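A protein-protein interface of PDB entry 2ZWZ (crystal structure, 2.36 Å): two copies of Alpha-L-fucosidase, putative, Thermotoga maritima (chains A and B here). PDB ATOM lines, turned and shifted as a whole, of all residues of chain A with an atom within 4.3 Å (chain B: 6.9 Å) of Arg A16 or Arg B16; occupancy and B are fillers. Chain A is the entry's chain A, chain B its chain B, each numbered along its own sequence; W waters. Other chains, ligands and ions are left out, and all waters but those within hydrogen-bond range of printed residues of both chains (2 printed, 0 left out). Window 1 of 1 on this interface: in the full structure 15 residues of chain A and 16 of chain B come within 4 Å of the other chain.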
ATOM      1  N   TRP A  12      10.222  11.844   4.481  1.00  0.00           N
ATOM      2  CA  TRP A  12       9.943  11.819   5.903  1.00  0.00           C
ATOM      3  C   TRP A  12       9.983  10.454   6.547  1.00  0.00           C
ATOM      4  O   TRP A  12      10.405  10.320   7.700  1.00  0.00           O
ATOM      5  CB  TRP A  12       8.615  12.476   6.164  1.00  0.00           C
ATOM      6  CG  TRP A  12       8.476  13.776   5.480  1.00  0.00           C
ATOM      7  CD1 TRP A  12       7.523  14.093   4.540  1.00  0.00           C
ATOM      8  CD2 TRP A  12       9.268  14.977   5.675  1.00  0.00           C
ATOM      9  NE1 TRP A  12       7.674  15.397   4.153  1.00  0.00           N
ATOM     10  CE2 TRP A  12       8.731  15.965   4.822  1.00  0.00           C
ATOM     11  CE3 TRP A  12      10.369  15.306   6.478  1.00  0.00           C
ATOM     12  CZ2 TRP A  12       9.270  17.281   4.736  1.00  0.00           C
ATOM     13  CZ3 TRP A  12      10.906  16.605   6.400  1.00  0.00           C
ATOM     14  CH2 TRP A  12      10.345  17.571   5.524  1.00  0.00           C
ATOM     15  N   GLU A  13       9.581   9.437   5.784  1.00  0.00           N
ATOM     16  CA  GLU A  13       9.549   8.074   6.275  1.00  0.00           C
ATOM     17  C   GLU A  13      10.954   7.576   6.548  1.00  0.00           C
ATOM     18  O   GLU A  13      11.183   6.869   7.506  1.00  0.00           O
ATOM     19  CB  GLU A  13       8.842   7.157   5.260  1.00  0.00           C
ATOM     20  CG  GLU A  13       8.315   5.916   5.923  1.00  0.00           C
ATOM     21  CD  GLU A  13       7.446   4.957   5.055  1.00  0.00           C
ATOM     22  OE1 GLU A  13       6.876   4.067   5.717  1.00  0.00           O
ATOM     23  OE2 GLU A  13       7.331   5.058   3.791  1.00  0.00           O
ATOM     24  N   SER A  14      11.897   7.929   5.698  1.00  0.00           N
ATOM     25  CA  SER A  14      13.294   7.519   5.889  1.00  0.00           C
ATOM     26  C   SER A  14      13.988   8.388   6.972  1.00  0.00           C
ATOM     27  O   SER A  14      14.764   7.887   7.808  1.00  0.00           O
ATOM     28  CB  SER A  14      14.062   7.694   4.577  1.00  0.00           C
ATOM     29  OG  SER A  14      15.466   7.713   4.821  1.00  0.00           O
ATOM     30  N   LEU A  15      13.707   9.692   6.930  1.00  0.00           N
ATOM     31  CA  LEU A  15      14.301  10.616   7.883  1.00  0.00           C
ATOM     32  C   LEU A  15      13.838  10.280   9.299  1.00  0.00           C
ATOM     33  O   LEU A  15      14.530  10.596  10.281  1.00  0.00           O
ATOM     34  CB  LEU A  15      13.994  12.100   7.539  1.00  0.00           C
ATOM     35  CG  LEU A  15      14.694  12.623   6.250  1.00  0.00           C
ATOM     36  CD1 LEU A  15      14.059  14.003   5.812  1.00  0.00           C
ATOM     37  CD2 LEU A  15      16.254  12.670   6.502  1.00  0.00           C
ATOM     38  N   ARG A  16      12.694   9.624   9.399  1.00  0.00           N
ATOM     39  CA  ARG A  16      12.166   9.222  10.709  1.00  0.00           C
ATOM     40  C   ARG A  16      13.132   8.245  11.477  1.00  0.00           C
ATOM     41  O   ARG A  16      13.082   8.142  12.683  1.00  0.00           O
ATOM     42  CB  ARG A  16      10.793   8.602  10.462  1.00  0.00           C
ATOM     43  CG  ARG A  16      10.224   7.743  11.575  1.00  0.00           C
ATOM     44  CD  ARG A  16       9.692   8.571  12.749  1.00  0.00           C
ATOM     45  NE  ARG A  16       8.990   7.757  13.738  1.00  0.00           N
ATOM     46  CZ  ARG A  16       8.539   8.226  14.897  1.00  0.00           C
ATOM     47  NH1 ARG A  16       8.749   9.486  15.191  1.00  0.00           N
ATOM     48  NH2 ARG A  16       7.845   7.433  15.736  1.00  0.00           N
ATOM     49  N   GLU A  17      14.018   7.570  10.747  1.00  0.00           N
ATOM     50  CA  GLU A  17      15.000   6.678  11.298  1.00  0.00           C
ATOM     51  C   GLU A  17      16.026   7.425  12.136  1.00  0.00           C
ATOM     52  O   GLU A  17      16.726   6.814  12.940  1.00  0.00           O
ATOM     53  CB  GLU A  17      15.749   5.948  10.179  1.00  0.00           C
ATOM     54  CG  GLU A  17      14.873   5.043   9.355  1.00  0.00           C
ATOM     55  CD  GLU A  17      15.619   4.454   8.207  1.00  0.00           C
ATOM     56  OE1 GLU A  17      15.003   3.931   7.248  1.00  0.00           O
ATOM     57  OE2 GLU A  17      16.859   4.509   8.273  1.00  0.00           O
ATOM     58  N   HIS A  18      16.185   8.723  11.905  1.00  0.00           N
ATOM     59  CA  HIS A  18      17.131   9.478  12.678  1.00  0.00           C
ATOM     60  C   HIS A  18      16.475   9.909  13.920  1.00  0.00           C
ATOM     61  O   HIS A  18      15.450  10.560  13.865  1.00  0.00           O
ATOM     62  CB  HIS A  18      17.592  10.722  11.945  1.00  0.00           C
ATOM     63  CG  HIS A  18      18.656  11.474  12.676  1.00  0.00           C
ATOM     64  ND1 HIS A  18      18.377  12.463  13.602  1.00  0.00           N
ATOM     65  CD2 HIS A  18      20.011  11.370  12.626  1.00  0.00           C
ATOM     66  CE1 HIS A  18      19.511  12.940  14.082  1.00  0.00           C
ATOM     67  NE2 HIS A  18      20.518  12.298  13.503  1.00  0.00           N
ATOM     68  N   PRO A 258       6.951  17.292   9.038  1.00  0.00           N
ATOM     69  CA  PRO A 258       6.881  16.038   9.816  1.00  0.00           C
ATOM     70  C   PRO A 258       8.055  15.735  10.725  1.00  0.00           C
ATOM     71  O   PRO A 258       7.846  15.351  11.846  1.00  0.00           O
ATOM     72  CB  PRO A 258       6.717  14.958   8.754  1.00  0.00           C
ATOM     73  CG  PRO A 258       5.848  15.664   7.724  1.00  0.00           C
ATOM     74  CD  PRO A 258       6.483  17.068   7.656  1.00  0.00           C
ATOM     75  N   HIS A 259       9.281  15.974  10.295  1.00  0.00           N
ATOM     76  CA  HIS A 259      10.467  15.638  11.099  1.00  0.00           C
ATOM     77  C   HIS A 259      11.006  16.659  12.096  1.00  0.00           C
ATOM     78  O   HIS A 259      10.854  17.885  11.912  1.00  0.00           O
ATOM     79  CB  HIS A 259      11.589  15.228  10.156  1.00  0.00           C
ATOM     80  CG  HIS A 259      12.742  14.555  10.846  1.00  0.00           C
ATOM     81  ND1 HIS A 259      12.651  13.291  11.391  1.00  0.00           N
ATOM     82  CD2 HIS A 259      13.990  14.999  11.139  1.00  0.00           C
ATOM     83  CE1 HIS A 259      13.786  12.985  11.987  1.00  0.00           C
ATOM     84  NE2 HIS A 259      14.615  14.005  11.848  1.00  0.00           N
ATOM     85  N   TRP A 260      11.612  16.127  13.167  1.00  0.00           N
ATOM     86  CA  TRP A 260      12.283  16.881  14.212  1.00  0.00           C
ATOM     87  C   TRP A 260      12.934  15.853  15.120  1.00  0.00           C
ATOM     88  O   TRP A 260      12.507  14.730  15.145  1.00  0.00           O
ATOM     89  CB  TRP A 260      11.318  17.805  14.991  1.00  0.00           C
ATOM     90  CG  TRP A 260      10.102  17.127  15.581  1.00  0.00           C
ATOM     91  CD1 TRP A 260       8.835  17.124  15.080  1.00  0.00           C
ATOM     92  CD2 TRP A 260      10.058  16.376  16.792  1.00  0.00           C
ATOM     93  NE1 TRP A 260       7.988  16.407  15.907  1.00  0.00           N
ATOM     94  CE2 TRP A 260       8.717  15.923  16.958  1.00  0.00           C
ATOM     95  CE3 TRP A 260      11.013  16.033  17.746  1.00  0.00           C
ATOM     96  CZ2 TRP A 260       8.311  15.135  18.044  1.00  0.00           C
ATOM     97  CZ3 TRP A 260      10.597  15.237  18.849  1.00  0.00           C
ATOM     98  CH2 TRP A 260       9.254  14.802  18.972  1.00  0.00           C
ATOM     99  N   ASP A 261      14.000  16.223  15.836  1.00  0.00           N
ATOM    100  CA  ASP A 261      14.691  15.277  16.724  1.00  0.00           C
ATOM    101  C   ASP A 261      14.360  15.612  18.196  1.00  0.00           C
ATOM    102  O   ASP A 261      14.473  14.757  19.064  1.00  0.00           O
ATOM    103  CB  ASP A 261      16.189  15.327  16.521  1.00  0.00           C
ATOM    104  CG  ASP A 261      16.610  14.824  15.172  1.00  0.00           C
ATOM    105  OD1 ASP A 261      17.421  15.533  14.511  1.00  0.00           O
ATOM    106  OD2 ASP A 261      16.173  13.702  14.761  1.00  0.00           O
ATOM    107  N   TYR B   8      -2.647  13.238  20.963  1.00  0.00           N
ATOM    108  CA  TYR B   8      -1.912  13.364  19.724  1.00  0.00           C
ATOM    109  C   TYR B   8      -2.898  14.044  18.757  1.00  0.00           C
ATOM    110  O   TYR B   8      -4.115  13.791  18.828  1.00  0.00           O
ATOM    111  CB  TYR B   8      -1.537  11.988  19.195  1.00  0.00           C
ATOM    112  CG  TYR B   8      -0.617  11.252  20.109  1.00  0.00           C
ATOM    113  CD1 TYR B   8       0.744  11.505  20.067  1.00  0.00           C
ATOM    114  CD2 TYR B   8      -1.121  10.336  21.054  1.00  0.00           C
ATOM    115  CE1 TYR B   8       1.619  10.859  20.952  1.00  0.00           C
ATOM    116  CE2 TYR B   8      -0.289   9.683  21.934  1.00  0.00           C
ATOM    117  CZ  TYR B   8       1.112   9.943  21.881  1.00  0.00           C
ATOM    118  OH  TYR B   8       2.023   9.255  22.687  1.00  0.00           O
ATOM    119  N   ASP B  11      -1.681  14.974  12.826  1.00  0.00           N
ATOM    120  CA  ASP B  11      -0.736  15.460  11.865  1.00  0.00           C
ATOM    121  C   ASP B  11       0.585  14.759  12.135  1.00  0.00           C
ATOM    122  O   ASP B  11       0.871  14.376  13.248  1.00  0.00           O
ATOM    123  CB  ASP B  11      -0.645  16.995  11.856  1.00  0.00           C
ATOM    124  CG  ASP B  11      -0.021  17.540  13.064  1.00  0.00           C
ATOM    125  OD1 ASP B  11      -0.752  18.064  13.946  1.00  0.00           O
ATOM    126  OD2 ASP B  11       1.221  17.452  13.132  1.00  0.00           O
ATOM    127  N   TRP B  12       1.358  14.509  11.081  1.00  0.00           N
ATOM    128  CA  TRP B  12       2.635  13.789  11.180  1.00  0.00           C
ATOM    129  C   TRP B  12       3.636  14.320  12.201  1.00  0.00           C
ATOM    130  O   TRP B  12       4.329  13.543  12.836  1.00  0.00           O
ATOM    131  CB  TRP B  12       3.308  13.721   9.802  1.00  0.00           C
ATOM    132  CG  TRP B  12       2.433  13.160   8.698  1.00  0.00           C
ATOM    133  CD1 TRP B  12       2.103  13.789   7.522  1.00  0.00           C
ATOM    134  CD2 TRP B  12       1.719  11.901   8.694  1.00  0.00           C
ATOM    135  NE1 TRP B  12       1.243  13.022   6.818  1.00  0.00           N
ATOM    136  CE2 TRP B  12       0.976  11.859   7.497  1.00  0.00           C
ATOM    137  CE3 TRP B  12       1.617  10.824   9.599  1.00  0.00           C
ATOM    138  CZ2 TRP B  12       0.122  10.772   7.162  1.00  0.00           C
ATOM    139  CZ3 TRP B  12       0.774   9.745   9.286  1.00  0.00           C
ATOM    140  CH2 TRP B  12       0.034   9.733   8.064  1.00  0.00           C
ATOM    141  N   GLU B  13       3.715  15.639  12.334  1.00  0.00           N
ATOM    142  CA  GLU B  13       4.622  16.308  13.253  1.00  0.00           C
ATOM    143  C   GLU B  13       4.210  15.952  14.700  1.00  0.00           C
ATOM    144  O   GLU B  13       5.049  15.692  15.552  1.00  0.00           O
ATOM    145  CB  GLU B  13       4.569  17.830  13.009  1.00  0.00           C
ATOM    146  CG  GLU B  13       5.704  18.573  13.651  1.00  0.00           C
ATOM    147  CD  GLU B  13       5.774  20.108  13.342  1.00  0.00           C
ATOM    148  OE1 GLU B  13       6.711  20.760  13.879  1.00  0.00           O
ATOM    149  OE2 GLU B  13       4.913  20.657  12.592  1.00  0.00           O
ATOM    150  N   SER B  14       2.922  15.947  14.969  1.00  0.00           N
ATOM    151  CA  SER B  14       2.465  15.592  16.276  1.00  0.00           C
ATOM    152  C   SER B  14       2.594  14.097  16.549  1.00  0.00           C
ATOM    153  O   SER B  14       3.076  13.713  17.622  1.00  0.00           O
ATOM    154  CB  SER B  14       1.011  16.008  16.440  1.00  0.00           C
ATOM    155  OG  SER B  14       0.455  15.384  17.585  1.00  0.00           O
ATOM    156  N   LEU B  15       2.183  13.256  15.573  1.00  0.00           N
ATOM    157  CA  LEU B  15       2.246  11.795  15.724  1.00  0.00           C
ATOM    158  C   LEU B  15       3.697  11.364  15.953  1.00  0.00           C
ATOM    159  O   LEU B  15       3.953  10.381  16.599  1.00  0.00           O
ATOM    160  CB  LEU B  15       1.671  11.109  14.502  1.00  0.00           C
ATOM    161  CG  LEU B  15       0.144  11.180  14.398  1.00  0.00           C
ATOM    162  CD1 LEU B  15      -0.335  10.799  12.976  1.00  0.00           C
ATOM    163  CD2 LEU B  15      -0.438  10.240  15.452  1.00  0.00           C
ATOM    164  N   ARG B  16       4.660  12.129  15.438  1.00  0.00           N
ATOM    165  CA  ARG B  16       6.079  11.787  15.661  1.00  0.00           C
ATOM    166  C   ARG B  16       6.446  11.788  17.170  1.00  0.00           C
ATOM    167  O   ARG B  16       7.396  11.188  17.540  1.00  0.00           O
ATOM    168  CB  ARG B  16       7.016  12.706  14.842  1.00  0.00           C
ATOM    169  CG  ARG B  16       8.354  13.004  15.554  1.00  0.00           C
ATOM    170  CD  ARG B  16       9.600  13.079  14.671  1.00  0.00           C
ATOM    171  NE  ARG B  16      10.162  11.746  14.398  1.00  0.00           N
ATOM    172  CZ  ARG B  16      11.439  11.379  14.544  1.00  0.00           C
ATOM    173  NH1 ARG B  16      12.407  12.207  14.981  1.00  0.00           N
ATOM    174  NH2 ARG B  16      11.756  10.149  14.211  1.00  0.00           N
ATOM    175  N   GLU B  17       5.681  12.469  18.025  1.00  0.00           N
ATOM    176  CA  GLU B  17       5.877  12.434  19.480  1.00  0.00           C
ATOM    177  C   GLU B  17       5.691  11.016  20.045  1.00  0.00           C
ATOM    178  O   GLU B  17       6.110  10.746  21.161  1.00  0.00           O
ATOM    179  CB  GLU B  17       4.866  13.338  20.180  1.00  0.00           C
ATOM    180  CG  GLU B  17       5.078  14.806  19.846  1.00  0.00           C
ATOM    181  CD  GLU B  17       4.019  15.727  20.414  1.00  0.00           C
ATOM    182  OE1 GLU B  17       3.948  16.877  19.948  1.00  0.00           O
ATOM    183  OE2 GLU B  17       3.242  15.305  21.300  1.00  0.00           O
ATOM    184  N   HIS B  18       5.039  10.121  19.313  1.00  0.00           N
ATOM    185  CA  HIS B  18       4.844   8.744  19.759  1.00  0.00           C
ATOM    186  C   HIS B  18       5.993   7.848  19.294  1.00  0.00           C
ATOM    187  O   HIS B  18       6.272   7.701  18.109  1.00  0.00           O
ATOM    188  CB  HIS B  18       3.498   8.205  19.233  1.00  0.00           C
ATOM    189  CG  HIS B  18       3.210   6.792  19.624  1.00  0.00           C
ATOM    190  ND1 HIS B  18       3.786   5.710  18.989  1.00  0.00           N
ATOM    191  CD2 HIS B  18       2.493   6.282  20.659  1.00  0.00           C
ATOM    192  CE1 HIS B  18       3.450   4.593  19.628  1.00  0.00           C
ATOM    193  NE2 HIS B  18       2.670   4.913  20.647  1.00  0.00           N
ATOM    194  N   THR B  19       6.721   7.269  20.212  1.00  0.00           N
ATOM    195  CA  THR B  19       7.776   6.375  19.765  1.00  0.00           C
ATOM    196  C   THR B  19       7.470   4.959  20.171  1.00  0.00           C
ATOM    197  O   THR B  19       6.494   4.708  20.905  1.00  0.00           O
ATOM    198  CB  THR B  19       9.074   6.792  20.317  1.00  0.00           C
ATOM    199  OG1 THR B  19       8.870   7.254  21.671  1.00  0.00           O
ATOM    200  CG2 THR B  19       9.604   7.915  19.454  1.00  0.00           C
ATOM    201  N   VAL B  20       8.268   4.022  19.659  1.00  0.00           N
ATOM    202  CA  VAL B  20       8.013   2.632  19.951  1.00  0.00           C
ATOM    203  C   VAL B  20       7.827   2.480  21.470  1.00  0.00           C
ATOM    204  O   VAL B  20       8.605   2.981  22.234  1.00  0.00           O
ATOM    205  CB  VAL B  20       9.164   1.754  19.418  1.00  0.00           C
ATOM    206  CG1 VAL B  20      10.489   2.076  20.166  1.00  0.00           C
ATOM    207  CG2 VAL B  20       8.801   0.289  19.540  1.00  0.00           C
ATOM    208  N   TYR B 243      -3.686   6.036  19.094  1.00  0.00           N
ATOM    209  CA  TYR B 243      -2.777   6.421  20.162  1.00  0.00           C
ATOM    210  C   TYR B 243      -3.501   7.155  21.284  1.00  0.00           C
ATOM    211  O   TYR B 243      -3.100   7.047  22.440  1.00  0.00           O
ATOM    212  CB  TYR B 243      -1.654   7.304  19.624  1.00  0.00           C
ATOM    213  CG  TYR B 243      -0.653   6.629  18.685  1.00  0.00           C
ATOM    214  CD1 TYR B 243      -0.219   5.278  18.879  1.00  0.00           C
ATOM    215  CD2 TYR B 243      -0.092   7.366  17.637  1.00  0.00           C
ATOM    216  CE1 TYR B 243       0.769   4.715  18.027  1.00  0.00           C
ATOM    217  CE2 TYR B 243       0.890   6.823  16.771  1.00  0.00           C
ATOM    218  CZ  TYR B 243       1.310   5.531  16.967  1.00  0.00           C
ATOM    219  OH  TYR B 243       2.288   5.097  16.114  1.00  0.00           O
ATOM    220  N   PRO B 258       4.554   8.994   6.446  1.00  0.00           N
ATOM    221  CA  PRO B 258       5.667   9.396   7.296  1.00  0.00           C
ATOM    222  C   PRO B 258       5.886   8.687   8.605  1.00  0.00           C
ATOM    223  O   PRO B 258       7.018   8.488   9.012  1.00  0.00           O
ATOM    224  CB  PRO B 258       5.425  10.868   7.505  1.00  0.00           C
ATOM    225  CG  PRO B 258       4.942  11.282   6.182  1.00  0.00           C
ATOM    226  CD  PRO B 258       3.919  10.184   5.848  1.00  0.00           C
ATOM    227  N   HIS B 259       4.824   8.270   9.257  1.00  0.00           N
ATOM    228  CA  HIS B 259       4.916   7.610  10.552  1.00  0.00           C
ATOM    229  C   HIS B 259       4.980   6.070  10.631  1.00  0.00           C
ATOM    230  O   HIS B 259       4.469   5.343   9.757  1.00  0.00           O
ATOM    231  CB  HIS B 259       3.759   8.128  11.395  1.00  0.00           C
ATOM    232  CG  HIS B 259       3.897   7.810  12.835  1.00  0.00           C
ATOM    233  ND1 HIS B 259       4.861   8.400  13.641  1.00  0.00           N
ATOM    234  CD2 HIS B 259       3.242   6.914  13.611  1.00  0.00           C
ATOM    235  CE1 HIS B 259       4.782   7.886  14.853  1.00  0.00           C
ATOM    236  NE2 HIS B 259       3.814   6.983  14.866  1.00  0.00           N
ATOM    237  N   TRP B 260       5.667   5.593  11.674  1.00  0.00           N
ATOM    238  CA  TRP B 260       5.816   4.165  12.017  1.00  0.00           C
ATOM    239  C   TRP B 260       6.538   4.151  13.360  1.00  0.00           C
ATOM    240  O   TRP B 260       7.242   5.090  13.700  1.00  0.00           O
ATOM    241  CB  TRP B 260       6.650   3.379  11.029  1.00  0.00           C
ATOM    242  CG  TRP B 260       8.002   4.026  10.596  1.00  0.00           C
ATOM    243  CD1 TRP B 260       8.208   4.852   9.496  1.00  0.00           C
ATOM    244  CD2 TRP B 260       9.291   3.907  11.242  1.00  0.00           C
ATOM    245  NE1 TRP B 260       9.526   5.242   9.428  1.00  0.00           N
ATOM    246  CE2 TRP B 260      10.217   4.686  10.475  1.00  0.00           C
ATOM    247  CE3 TRP B 260       9.751   3.240  12.396  1.00  0.00           C
ATOM    248  CZ2 TRP B 260      11.561   4.808  10.822  1.00  0.00           C
ATOM    249  CZ3 TRP B 260      11.079   3.367  12.745  1.00  0.00           C
ATOM    250  CH2 TRP B 260      11.978   4.150  11.954  1.00  0.00           C
ATOM    251  N   ASP B 261       6.380   3.095  14.122  1.00  0.00           N
ATOM    252  CA  ASP B 261       7.057   2.996  15.417  1.00  0.00           C
ATOM    253  C   ASP B 261       8.267   2.050  15.316  1.00  0.00           C
ATOM    254  O   ASP B 261       9.210   2.172  16.086  1.00  0.00           O
ATOM    255  CB  ASP B 261       6.076   2.477  16.477  1.00  0.00           C
ATOM    256  CG  ASP B 261       5.025   3.503  16.831  1.00  0.00           C
ATOM    257  OD1 ASP B 261       3.823   3.153  16.805  1.00  0.00           O
ATOM    258  OD2 ASP B 261       5.407   4.669  17.133  1.00  0.00           O
ATOM    259  N   PHE B 262       8.191   1.071  14.412  1.00  0.00           N
ATOM    260  CA  PHE B 262       9.287   0.120  14.169  1.00  0.00           C
ATOM    261  C   PHE B 262       9.238  -0.323  12.739  1.00  0.00           C
ATOM    262  O   PHE B 262       8.141  -0.377  12.119  1.00  0.00           O
ATOM    263  CB  PHE B 262       9.210  -1.110  15.077  1.00  0.00           C
ATOM    264  CG  PHE B 262       7.947  -1.902  14.938  1.00  0.00           C
ATOM    265  CD1 PHE B 262       7.887  -2.984  14.086  1.00  0.00           C
ATOM    266  CD2 PHE B 262       6.807  -1.591  15.725  1.00  0.00           C
ATOM    267  CE1 PHE B 262       6.733  -3.757  14.016  1.00  0.00           C
ATOM    268  CE2 PHE B 262       5.669  -2.364  15.645  1.00  0.00           C
ATOM    269  CZ  PHE B 262       5.640  -3.456  14.783  1.00  0.00           C
ATOM    270  N   GLY B 277      19.972   1.520  14.012  1.00  0.00           N
ATOM    271  CA  GLY B 277      19.763   2.835  14.596  1.00  0.00           C
ATOM    272  C   GLY B 277      18.336   3.281  14.888  1.00  0.00           C
ATOM    273  O   GLY B 277      18.076   4.474  15.230  1.00  0.00           O
ATOM    274  N   TYR B 278      17.402   2.343  14.717  1.00  0.00           N
ATOM    275  CA  TYR B 278      15.973   2.575  14.995  1.00  0.00           C
ATOM    276  C   TYR B 278      15.474   1.204  15.346  1.00  0.00           C
ATOM    277  O   TYR B 278      16.143   0.231  15.088  1.00  0.00           O
ATOM    278  CB  TYR B 278      15.237   3.104  13.750  1.00  0.00           C
ATOM    279  CG  TYR B 278      15.576   2.337  12.500  1.00  0.00           C
ATOM    280  CD1 TYR B 278      14.986   1.118  12.219  1.00  0.00           C
ATOM    281  CD2 TYR B 278      16.548   2.804  11.630  1.00  0.00           C
ATOM    282  CE1 TYR B 278      15.367   0.376  11.099  1.00  0.00           C
ATOM    283  CE2 TYR B 278      16.917   2.087  10.534  1.00  0.00           C
ATOM    284  CZ  TYR B 278      16.341   0.884  10.272  1.00  0.00           C
ATOM    285  OH  TYR B 278      16.785   0.162   9.194  1.00  0.00           O
HETATM  286  O   HOH W   1       4.943   3.386   7.264  1.00  0.00           O
HETATM  287  O   HOH W   2       9.717  20.534  12.662  1.00  0.00           O
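The backbone carbonyl oxygen (O) of Glu A13 lies within hydrogen-bond range of the indole nitrogen (NE1) of Trp B260, 3.0 Å away. The guanidinium group (NH2) of Arg B16 sits at hydrogen-bond distance from the backbone carbonyl oxygen (O) of Arg A16, 2.8 Å away. The guanidinium group (NH2) of Arg A16 is in hydrogen-bond range of the backbone carbonyl oxygen (O) of His B18, 2.9 Å away. The backbone carbonyl oxygen (O) of Trp B260 sits at hydrogen-bond distance from the guanidinium group (NH2) of Arg A16 (3.2 Å). The guanidinium group of Arg A16 is in salt-bridge range of the side-chain carboxylate of Asp B261 (3.9 Å). The backbone carbonyl oxygen (O) of Glu B13 lies within hydrogen-bond range of the indole nitrogen (NE1) of Trp A260, 3.0 Å away. NH1 of Arg B16 sits at hydrogen-bond distance from O of Trp A260, at 2.5 Å.
The backbone carbonyl oxygen of Leu A15 lies close to a ring nitrogen (ND1) of His A259 (3.5 Å). The side-chain carboxylate (OD2) of Asp A261 is in hydrogen-bond range of a ring nitrogen (ND1) of His A18, at 2.8 Å. OD2 of Asp A261 is in hydrogen-bond range of NE2 of His A259 (3.3 Å). A ring nitrogen (ND1) of His B18 sits at hydrogen-bond distance from the side-chain carboxylate of Asp B261, 2.7 Å away. OH of Tyr B243 sits at hydrogen-bond distance from NE2 of His B259 (2.7 Å). The side-chain hydroxyl of Tyr B243 is in hydrogen-bond range of the side-chain carboxylate of Asp B261 (2.6 Å).
Among the printed residues, merely in contact across the chains: Trp A12 with Pro B258 (3.8 Å), Glu A13 with Pro B258 (3.8 Å), Arg A16 with His B259 (3.2 Å), Glu A17 with Trp B260 (3.6 Å), Glu A17 with Gly B277 (3.5 Å), Glu A17 with Tyr B278 (3.3 Å), His A18 with Arg B16 (3.6 Å), Pro A258 with Trp B12 (3.8 Å), Pro A258 with Glu B13 (3.6 Å), His A259 with Arg B16 (3.4 Å) and Trp A260 with Glu B17 (3.7 Å).
Arg A16 touches five residues of chain B. Of the printed residues of chain B, Pro A258 touches Trp B12 (3.8 Å) and Glu B13 (3.6 Å). Arg B16 touches just these residues of chain A: Arg A16 (2.8 Å), His A18 (3.6 Å), His A259 (3.4 Å) and Trp A260 (2.5 Å). Printed residues of chain A within 4 Å of Glu B17: Trp A260. Printed residues of chain A within 4 Å of His B259: Arg A16 (3.2 Å). The nearest residue of chain A that does not touch Arg B16 is Pro A258 (4.03 Å). The nearest printed residue of chain B that does not touch Glu A17 is Arg B16 (4.9 Å).
Printed residues of chain A that touch a printed residue of chain B: Trp A12, Glu A13, Arg A16, Glu A17, His A18, Pro A258, His A259 and Trp A260. Hydrophobic or aromatic side chains of chain A that line the printed part of chain B: Trp A12, Pro A258, His A259 and Trp A260. Along chain A the printed residues that touch a printed residue of chain B span positions 12 to 260. Among the printed residues, Asp or Glu carboxylates within 4 Å of a Lys or Arg side-chain nitrogen of the other chain: Arg A16 with Asp B261 (3.9 Å).
Trp A12 touches Pro B258, and with the chains exchanged Pro A258 touches Trp B12. Glu A13 touches Pro B258, and with the chains exchanged Pro A258 touches Glu B13. Arg A16 touches its own counterpart, Arg B16. Arg A16 touches Asp B261, but with the chains exchanged Asp A261 does not touch Arg B16 (4.1 Å). Positions printed for both chains: 12, 13, 14, 15, 16, 17, 18, 258, 259, 260 and 261.
Water W1 bridges OE1 of Glu A13 (2.6 Å) and O of His B259 (3.2 Å). Water W2 lies within hydrogen-bond range of O of His A259 (3.0 Å) and OE1 of Glu B13 (3.3 Å).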
